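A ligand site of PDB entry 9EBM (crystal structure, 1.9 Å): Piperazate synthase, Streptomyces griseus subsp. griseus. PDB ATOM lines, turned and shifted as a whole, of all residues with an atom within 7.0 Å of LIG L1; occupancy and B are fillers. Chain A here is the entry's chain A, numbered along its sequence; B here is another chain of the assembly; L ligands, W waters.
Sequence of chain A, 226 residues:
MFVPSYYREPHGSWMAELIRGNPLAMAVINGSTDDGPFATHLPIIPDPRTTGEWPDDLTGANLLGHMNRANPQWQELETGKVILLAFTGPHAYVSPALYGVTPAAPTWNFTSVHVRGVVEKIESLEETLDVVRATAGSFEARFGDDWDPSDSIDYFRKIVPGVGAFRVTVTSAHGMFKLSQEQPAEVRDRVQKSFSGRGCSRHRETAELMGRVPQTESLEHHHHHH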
ATOM      1  N   PRO A  43     -16.222 -18.437   3.885  1.00  0.00           N
ATOM      2  CA  PRO A  43     -17.106 -19.584   4.144  1.00  0.00           C
ATOM      3  C   PRO A  43     -18.272 -19.642   3.170  1.00  0.00           C
ATOM      4  O   PRO A  43     -18.904 -18.619   2.882  1.00  0.00           O
ATOM      5  CB  PRO A  43     -17.586 -19.358   5.580  1.00  0.00           C
ATOM      6  CG  PRO A  43     -17.660 -17.815   5.692  1.00  0.00           C
ATOM      7  CD  PRO A  43     -16.471 -17.323   4.837  1.00  0.00           C
ATOM      8  N   HIS A  66     -19.706 -14.826   2.176  1.00  0.00           N
ATOM      9  CA  HIS A  66     -19.538 -13.429   2.543  1.00  0.00           C
ATOM     10  C   HIS A  66     -18.049 -13.139   2.667  1.00  0.00           C
ATOM     11  O   HIS A  66     -17.234 -14.036   2.896  1.00  0.00           O
ATOM     12  CB  HIS A  66     -20.323 -13.041   3.828  1.00  0.00           C
ATOM     13  CG  HIS A  66     -19.734 -13.533   5.124  1.00  0.00           C
ATOM     14  ND1 HIS A  66     -19.913 -14.823   5.579  1.00  0.00           N
ATOM     15  CD2 HIS A  66     -19.024 -12.889   6.085  1.00  0.00           C
ATOM     16  CE1 HIS A  66     -19.321 -14.957   6.758  1.00  0.00           C
ATOM     17  NE2 HIS A  66     -18.780 -13.801   7.090  1.00  0.00           N
ATOM     18  N   VAL A 132     -25.118 -14.538   7.143  1.00  0.00           N
ATOM     19  CA  VAL A 132     -24.114 -14.843   8.169  1.00  0.00           C
ATOM     20  C   VAL A 132     -24.736 -15.630   9.312  1.00  0.00           C
ATOM     21  O   VAL A 132     -24.061 -16.465   9.924  1.00  0.00           O
ATOM     22  CB  VAL A 132     -23.423 -13.567   8.680  1.00  0.00           C
ATOM     23  CG1 VAL A 132     -22.680 -12.865   7.573  1.00  0.00           C
ATOM     24  CG2 VAL A 132     -24.435 -12.639   9.345  1.00  0.00           C
ATOM     25  N   TYR A 155     -25.256  -8.224  18.561  1.00  0.00           N
ATOM     26  CA  TYR A 155     -23.889  -8.022  18.099  1.00  0.00           C
ATOM     27  C   TYR A 155     -23.784  -8.227  16.600  1.00  0.00           C
ATOM     28  O   TYR A 155     -23.112  -7.456  15.907  1.00  0.00           O
ATOM     29  CB  TYR A 155     -22.936  -8.953  18.844  1.00  0.00           C
ATOM     30  CG  TYR A 155     -21.511  -8.924  18.331  1.00  0.00           C
ATOM     31  CD1 TYR A 155     -20.734  -7.768  18.433  1.00  0.00           C
ATOM     32  CD2 TYR A 155     -20.924 -10.056  17.770  1.00  0.00           C
ATOM     33  CE1 TYR A 155     -19.416  -7.747  17.966  1.00  0.00           C
ATOM     34  CE2 TYR A 155     -19.631 -10.043  17.317  1.00  0.00           C
ATOM     35  CZ  TYR A 155     -18.874  -8.890  17.411  1.00  0.00           C
ATOM     36  OH  TYR A 155     -17.573  -8.904  16.951  1.00  0.00           O
ATOM     37  N   ILE A 159     -22.397  -5.362  13.552  1.00  0.00           N
ATOM     38  CA  ILE A 159     -21.254  -5.501  12.635  1.00  0.00           C
ATOM     39  C   ILE A 159     -21.656  -5.927  11.242  1.00  0.00           C
ATOM     40  O   ILE A 159     -20.808  -5.879  10.327  1.00  0.00           O
ATOM     41  CB  ILE A 159     -20.192  -6.472  13.211  1.00  0.00           C
ATOM     42  CG1 ILE A 159     -20.668  -7.928  13.172  1.00  0.00           C
ATOM     43  CG2 ILE A 159     -19.848  -6.079  14.637  1.00  0.00           C
ATOM     44  CD1 ILE A 159     -19.567  -8.925  13.538  1.00  0.00           C
ATOM     45  N   VAL A 163     -20.312  -6.583   6.232  1.00  0.00           N
ATOM     46  CA  VAL A 163     -20.363  -7.863   5.537  1.00  0.00           C
ATOM     47  C   VAL A 163     -20.700  -7.635   4.074  1.00  0.00           C
ATOM     48  O   VAL A 163     -21.656  -6.938   3.742  1.00  0.00           O
ATOM     49  CB  VAL A 163     -21.405  -8.794   6.175  1.00  0.00           C
ATOM     50  CG1 VAL A 163     -21.512 -10.105   5.359  1.00  0.00           C
ATOM     51  CG2 VAL A 163     -21.035  -9.087   7.611  1.00  0.00           C
ATOM     52  N   TYR B   6      -3.471  -7.556  11.576  1.00  0.00           N
ATOM     53  CA  TYR B   6      -3.159  -8.412  12.699  1.00  0.00           C
ATOM     54  C   TYR B   6      -3.079  -9.887  12.309  1.00  0.00           C
ATOM     55  O   TYR B   6      -2.713 -10.708  13.157  1.00  0.00           O
ATOM     56  CB  TYR B   6      -4.178  -8.222  13.834  1.00  0.00           C
ATOM     57  CG  TYR B   6      -5.588  -7.963  13.369  1.00  0.00           C
ATOM     58  CD1 TYR B   6      -6.463  -9.021  13.127  1.00  0.00           C
ATOM     59  CD2 TYR B   6      -6.053  -6.658  13.149  1.00  0.00           C
ATOM     60  CE1 TYR B   6      -7.767  -8.783  12.699  1.00  0.00           C
ATOM     61  CE2 TYR B   6      -7.353  -6.423  12.713  1.00  0.00           C
ATOM     62  CZ  TYR B   6      -8.204  -7.489  12.486  1.00  0.00           C
ATOM     63  OH  TYR B   6      -9.493  -7.282  12.055  1.00  0.00           O
ATOM     64  N   TYR B   7      -3.404 -10.221  11.059  1.00  0.00           N
ATOM     65  CA  TYR B   7      -3.284 -11.588  10.571  1.00  0.00           C
ATOM     66  C   TYR B   7      -2.073 -11.803   9.662  1.00  0.00           C
ATOM     67  O   TYR B   7      -1.884 -12.925   9.162  1.00  0.00           O
ATOM     68  CB  TYR B   7      -4.558 -12.002   9.817  1.00  0.00           C
ATOM     69  CG  TYR B   7      -5.789 -12.054  10.688  1.00  0.00           C
ATOM     70  CD1 TYR B   7      -5.726 -12.483  12.006  1.00  0.00           C
ATOM     71  CD2 TYR B   7      -7.025 -11.696  10.182  1.00  0.00           C
ATOM     72  CE1 TYR B   7      -6.866 -12.534  12.814  1.00  0.00           C
ATOM     73  CE2 TYR B   7      -8.168 -11.740  10.962  1.00  0.00           C
ATOM     74  CZ  TYR B   7      -8.081 -12.160  12.264  1.00  0.00           C
ATOM     75  OH  TYR B   7      -9.236 -12.203  13.025  1.00  0.00           O
ATOM     76  N   TYR B  99     -14.809 -19.362  23.782  1.00  0.00           N
ATOM     77  CA  TYR B  99     -14.405 -18.015  24.180  1.00  0.00           C
ATOM     78  C   TYR B  99     -14.653 -17.778  25.667  1.00  0.00           C
ATOM     79  O   TYR B  99     -13.777 -17.251  26.366  1.00  0.00           O
ATOM     80  CB  TYR B  99     -15.147 -16.978  23.340  1.00  0.00           C
ATOM     81  CG  TYR B  99     -14.675 -16.887  21.896  1.00  0.00           C
ATOM     82  CD1 TYR B  99     -13.552 -17.577  21.458  1.00  0.00           C
ATOM     83  CD2 TYR B  99     -15.342 -16.079  20.988  1.00  0.00           C
ATOM     84  CE1 TYR B  99     -13.122 -17.474  20.143  1.00  0.00           C
ATOM     85  CE2 TYR B  99     -14.920 -15.970  19.690  1.00  0.00           C
ATOM     86  CZ  TYR B  99     -13.818 -16.670  19.259  1.00  0.00           C
ATOM     87  OH  TYR B  99     -13.417 -16.551  17.959  1.00  0.00           O
ATOM     88  N   PRO B 103     -20.906 -10.787  23.816  1.00  0.00           N
ATOM     89  CA  PRO B 103     -21.314 -11.590  22.667  1.00  0.00           C
ATOM     90  C   PRO B 103     -20.135 -11.996  21.800  1.00  0.00           C
ATOM     91  O   PRO B 103     -19.002 -11.597  22.072  1.00  0.00           O
ATOM     92  CB  PRO B 103     -22.242 -10.651  21.908  1.00  0.00           C
ATOM     93  CG  PRO B 103     -21.607  -9.304  22.122  1.00  0.00           C
ATOM     94  CD  PRO B 103     -21.000  -9.347  23.519  1.00  0.00           C
ATOM     95  N   ALA B 104     -20.393 -12.783  20.754  1.00  0.00           N
ATOM     96  CA  ALA B 104     -19.318 -13.242  19.883  1.00  0.00           C
ATOM     97  C   ALA B 104     -19.926 -13.731  18.582  1.00  0.00           C
ATOM     98  O   ALA B 104     -21.136 -13.896  18.459  1.00  0.00           O
ATOM     99  CB  ALA B 104     -18.484 -14.333  20.552  1.00  0.00           C
ATOM    100  N   ALA B 105     -19.057 -13.954  17.602  1.00  0.00           N
ATOM    101  CA  ALA B 105     -19.437 -14.618  16.370  1.00  0.00           C
ATOM    102  C   ALA B 105     -18.401 -15.694  16.105  1.00  0.00           C
ATOM    103  O   ALA B 105     -17.245 -15.550  16.509  1.00  0.00           O
ATOM    104  CB  ALA B 105     -19.506 -13.644  15.186  1.00  0.00           C
ATOM    105  N   PRO B 106     -18.781 -16.797  15.458  1.00  0.00           N
ATOM    106  CA  PRO B 106     -17.797 -17.840  15.176  1.00  0.00           C
ATOM    107  C   PRO B 106     -16.834 -17.360  14.107  1.00  0.00           C
ATOM    108  O   PRO B 106     -17.040 -16.326  13.474  1.00  0.00           O
ATOM    109  CB  PRO B 106     -18.638 -19.032  14.673  1.00  0.00           C
ATOM    110  CG  PRO B 106     -20.059 -18.626  14.822  1.00  0.00           C
ATOM    111  CD  PRO B 106     -20.088 -17.119  14.863  1.00  0.00           C
ATOM    112  N   THR B 107     -15.786 -18.136  13.909  1.00  0.00           N
ATOM    113  CA  THR B 107     -14.858 -17.843  12.831  1.00  0.00           C
ATOM    114  C   THR B 107     -14.142 -19.135  12.463  1.00  0.00           C
ATOM    115  O   THR B 107     -14.417 -20.202  13.015  1.00  0.00           O
ATOM    116  CB  THR B 107     -13.899 -16.718  13.230  1.00  0.00           C
ATOM    117  OG1 THR B 107     -13.300 -16.162  12.055  1.00  0.00           O
ATOM    118  CG2 THR B 107     -12.807 -17.237  14.176  1.00  0.00           C
ATOM    119  N   TRP B 108     -13.252 -19.033  11.473  1.00  0.00           N
ATOM    120  CA  TRP B 108     -12.454 -20.156  11.013  1.00  0.00           C
ATOM    121  C   TRP B 108     -11.018 -19.694  11.025  1.00  0.00           C
ATOM    122  O   TRP B 108     -10.661 -18.769  10.289  1.00  0.00           O
ATOM    123  CB  TRP B 108     -12.878 -20.618   9.614  1.00  0.00           C
ATOM    124  CG  TRP B 108     -12.575 -22.074   9.351  1.00  0.00           C
ATOM    125  CD1 TRP B 108     -11.329 -22.654   9.262  1.00  0.00           C
ATOM    126  CD2 TRP B 108     -13.520 -23.129   9.180  1.00  0.00           C
ATOM    127  NE1 TRP B 108     -11.449 -24.005   9.019  1.00  0.00           N
ATOM    128  CE2 TRP B 108     -12.785 -24.321   8.970  1.00  0.00           C
ATOM    129  CE3 TRP B 108     -14.926 -23.190   9.166  1.00  0.00           C
ATOM    130  CZ2 TRP B 108     -13.406 -25.562   8.754  1.00  0.00           C
ATOM    131  CZ3 TRP B 108     -15.534 -24.413   8.960  1.00  0.00           C
ATOM    132  CH2 TRP B 108     -14.770 -25.584   8.756  1.00  0.00           C
ATOM    133  N   LYS B 178      -4.578 -16.411  10.189  1.00  0.00           N
ATOM    134  CA  LYS B 178      -5.748 -16.067  10.991  1.00  0.00           C
ATOM    135  C   LYS B 178      -5.749 -16.993  12.192  1.00  0.00           C
ATOM    136  O   LYS B 178      -6.166 -18.153  12.090  1.00  0.00           O
ATOM    137  CB  LYS B 178      -7.023 -16.181  10.155  1.00  0.00           C
ATOM    138  CG  LYS B 178      -8.255 -15.501  10.793  1.00  0.00           C
ATOM    139  CD  LYS B 178      -9.481 -15.654   9.879  1.00  0.00           C
ATOM    140  CE  LYS B 178     -10.672 -14.842  10.373  1.00  0.00           C
ATOM    141  NZ  LYS B 178     -10.800 -15.099  11.809  1.00  0.00           N
ATOM    142  N   GLU B 182      -7.151 -11.336  16.968  1.00  0.00           N
ATOM    143  CA  GLU B 182      -8.120 -10.306  17.335  1.00  0.00           C
ATOM    144  C   GLU B 182      -8.704 -10.497  18.743  1.00  0.00           C
ATOM    145  O   GLU B 182      -9.407  -9.606  19.219  1.00  0.00           O
ATOM    146  CB  GLU B 182      -9.255 -10.264  16.310  1.00  0.00           C
ATOM    147  CG  GLU B 182     -10.418 -11.210  16.571  1.00  0.00           C
ATOM    148  CD  GLU B 182     -10.171 -12.621  16.057  1.00  0.00           C
ATOM    149  OE1 GLU B 182     -11.121 -13.450  16.110  1.00  0.00           O
ATOM    150  OE2 GLU B 182      -9.042 -12.900  15.601  1.00  0.00           O
ATOM    151  N   GLN B 183      -8.418 -11.617  19.417  1.00  0.00           N
ATOM    152  CA  GLN B 183      -9.014 -11.915  20.709  1.00  0.00           C
ATOM    153  C   GLN B 183      -8.027 -11.672  21.849  1.00  0.00           C
ATOM    154  O   GLN B 183      -6.815 -11.643  21.625  1.00  0.00           O
ATOM    155  CB  GLN B 183      -9.476 -13.372  20.761  1.00  0.00           C
ATOM    156  CG  GLN B 183     -10.465 -13.739  19.673  1.00  0.00           C
ATOM    157  CD  GLN B 183     -11.844 -13.152  19.932  1.00  0.00           C
ATOM    158  OE1 GLN B 183     -12.225 -12.907  21.073  1.00  0.00           O
ATOM    159  NE2 GLN B 183     -12.591 -12.912  18.858  1.00  0.00           N
HETATM  160  C1  LIG L   1     -15.517 -11.019  15.354  1.00  0.00           C
HETATM  161  N1  LIG L   1     -14.318  -9.911  13.460  1.00  0.00           N
HETATM  162  O1  LIG L   1     -14.387 -11.532  15.442  1.00  0.00           O
HETATM  163  C2  LIG L   1     -15.739 -10.262  13.887  1.00  0.00           C
HETATM  164  C3  LIG L   1     -16.469 -11.138  12.849  1.00  0.00           C
HETATM  165  C4  LIG L   1     -16.898 -13.524  12.193  1.00  0.00           C
HETATM  166  N2  LIG L   1     -16.892 -13.299  10.698  1.00  0.00           N
HETATM  167  C5  LIG L   1     -15.883 -12.552  12.805  1.00  0.00           C
HETATM  168  O2  LIG L   1     -15.612 -13.042  10.361  1.00  0.00           O
HETATM  169  O3  LIG L   1     -16.491 -10.960  16.101  1.00  0.00           O
HETATM  170  C1  LG2 L   2     -15.513 -11.294   7.310  1.00  0.00           C
HETATM  171  C2  LG2 L   2     -15.547 -16.112   8.150  1.00  0.00           C
HETATM  172  C3  LG2 L   2     -19.784 -15.563  10.512  1.00  0.00           C
HETATM  173  C4  LG2 L   2     -19.423 -10.767  10.131  1.00  0.00           C
HETATM  174  C5  LG2 L   2     -15.147 -12.638   7.317  1.00  0.00           C
HETATM  175  C6  LG2 L   2     -13.983 -13.224   6.700  1.00  0.00           C
HETATM  176  C7  LG2 L   2     -13.996 -14.545   6.940  1.00  0.00           C
HETATM  177  C8  LG2 L   2     -15.177 -14.855   7.708  1.00  0.00           C
HETATM  178  C9  LG2 L   2     -12.973 -15.605   6.493  1.00  0.00           C
HETATM  179  C10 LG2 L   2     -12.893 -12.449   5.902  1.00  0.00           C
HETATM  180  C11 LG2 L   2     -13.355 -12.385   4.447  1.00  0.00           C
HETATM  181  C12 LG2 L   2     -12.342 -11.634   3.622  1.00  0.00           C
HETATM  182  O1  LG2 L   2     -11.123 -11.973   3.667  1.00  0.00           O
HETATM  183  O2  LG2 L   2     -12.786 -10.720   2.887  1.00  0.00           O
HETATM  184  C13 LG2 L   2     -16.685 -16.371   8.881  1.00  0.00           C
HETATM  185  C14 LG2 L   2     -17.110 -17.668   9.386  1.00  0.00           C
HETATM  186  C15 LG2 L   2     -18.293 -17.510  10.010  1.00  0.00           C
HETATM  187  C16 LG2 L   2     -18.641 -16.106   9.950  1.00  0.00           C
HETATM  188  C17 LG2 L   2     -16.278 -18.957   9.146  1.00  0.00           C
HETATM  189  C18 LG2 L   2     -19.215 -18.512  10.750  1.00  0.00           C
HETATM  190  C19 LG2 L   2     -18.860 -19.755  11.080  1.00  0.00           C
HETATM  191  C20 LG2 L   2     -20.083 -14.223  10.647  1.00  0.00           C
HETATM  192  C21 LG2 L   2     -21.199 -13.636  11.383  1.00  0.00           C
HETATM  193  C22 LG2 L   2     -21.110 -12.307  11.261  1.00  0.00           C
HETATM  194  C23 LG2 L   2     -19.914 -12.006  10.481  1.00  0.00           C
HETATM  195  C24 LG2 L   2     -22.310 -14.423  12.129  1.00  0.00           C
HETATM  196  C25 LG2 L   2     -22.091 -11.271  11.859  1.00  0.00           C
HETATM  197  C26 LG2 L   2     -22.385 -10.177  11.145  1.00  0.00           C
HETATM  198  C27 LG2 L   2     -18.308 -10.479   9.376  1.00  0.00           C
HETATM  199  C28 LG2 L   2     -17.756  -9.159   9.129  1.00  0.00           C
HETATM  200  C29 LG2 L   2     -16.673  -9.310   8.355  1.00  0.00           C
HETATM  201  C30 LG2 L   2     -16.512 -10.726   8.065  1.00  0.00           C
HETATM  202  C31 LG2 L   2     -18.335  -7.840   9.684  1.00  0.00           C
HETATM  203  C32 LG2 L   2     -15.736  -8.199   7.803  1.00  0.00           C
HETATM  204  C33 LG2 L   2     -14.964  -7.428   8.872  1.00  0.00           C
HETATM  205  C34 LG2 L   2     -14.534  -8.340   9.994  1.00  0.00           C
HETATM  206  O3  LG2 L   2     -14.857  -8.015  11.166  1.00  0.00           O
HETATM  207  O4  LG2 L   2     -13.877  -9.375   9.702  1.00  0.00           O
HETATM  208  N1  LG2 L   2     -15.838 -13.665   7.919  1.00  0.00           N
HETATM  209  N2  LG2 L   2     -17.647 -15.447   9.238  1.00  0.00           N
HETATM  210  N3  LG2 L   2     -19.327 -13.197  10.137  1.00  0.00           N
HETATM  211  N4  LG2 L   2     -17.525 -11.409   8.718  1.00  0.00           N
HETATM  212 FE1  LG2 L   2     -17.659 -13.484   8.888  1.00  0.00          FE
HETATM  213  O   HOH W   1     -12.753 -11.798  10.312  1.00  0.00           O
HETATM  214  O   HOH W   2     -16.465 -12.709  18.174  1.00  0.00           O
HETATM  215  O   HOH W   3     -11.513 -10.410  12.412  1.00  0.00           O
HETATM  216  O   HOH W   4     -11.885  -8.191  14.000  1.00  0.00           O
HETATM  217  O   HOH W   5     -15.479  -7.387  15.374  1.00  0.00           O
HETATM  218  O   HOH W   6     -14.765 -14.719  16.474  1.00  0.00           O
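OH of Tyr 155 is in hydrogen-bond range of O3 of LIG L1, at 2.5 Å. FE1 of LG2 L2 is bound by NE2 of His 66.
A nitrogen (N2) of LIG L1 is bound to an iron atom (FE1) of LG2 L2, at 2.0 Å.
OE1 of Glu 182 of chain B sits at hydrogen-bond distance from NE2 of Gln 183 of chain B (3.2 Å).
Residues that only touch LIG L1: Pro 106 of chain B (3.1 Å), Glu 182 of chain B (3.8 Å), Ile 159 (3.9 Å) and Ala 105 of chain B (3.97 Å). Hydrophobic or aromatic side chains within 4 Å of LIG L1: Tyr 155, Ile 159 and Ala 105 of chain B. Within 4 Å of LIG L1: Tyr 155, Ile 159, Ala 105 of chain B, Pro 106 of chain B and Glu 182 of chain B. The nearest printed residue that does not touch LIG L1 is Gln 183 of chain B (4.1 Å).
Water W2 bridges an oxygen (O3) of LIG L1 (2.7 Å) and the backbone NH (N) of Ala 105 of chain B (2.9 Å). Water W4 lies within hydrogen-bond range of a nitrogen (N1) of LIG L1 (3.0 Å) and the side-chain hydroxyl of Tyr 6 of chain B (3.2 Å). Water W5 lies within hydrogen-bond range of OH of Tyr 155 (3.0 Å) and N1 of LIG L1 (3.4 Å). Water W6 lies within hydrogen-bond range of the backbone carbonyl oxygen of Ala 105 of chain B, the side-chain hydroxyl of Tyr 99 of chain B and an oxygen (O1) of LIG L1.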
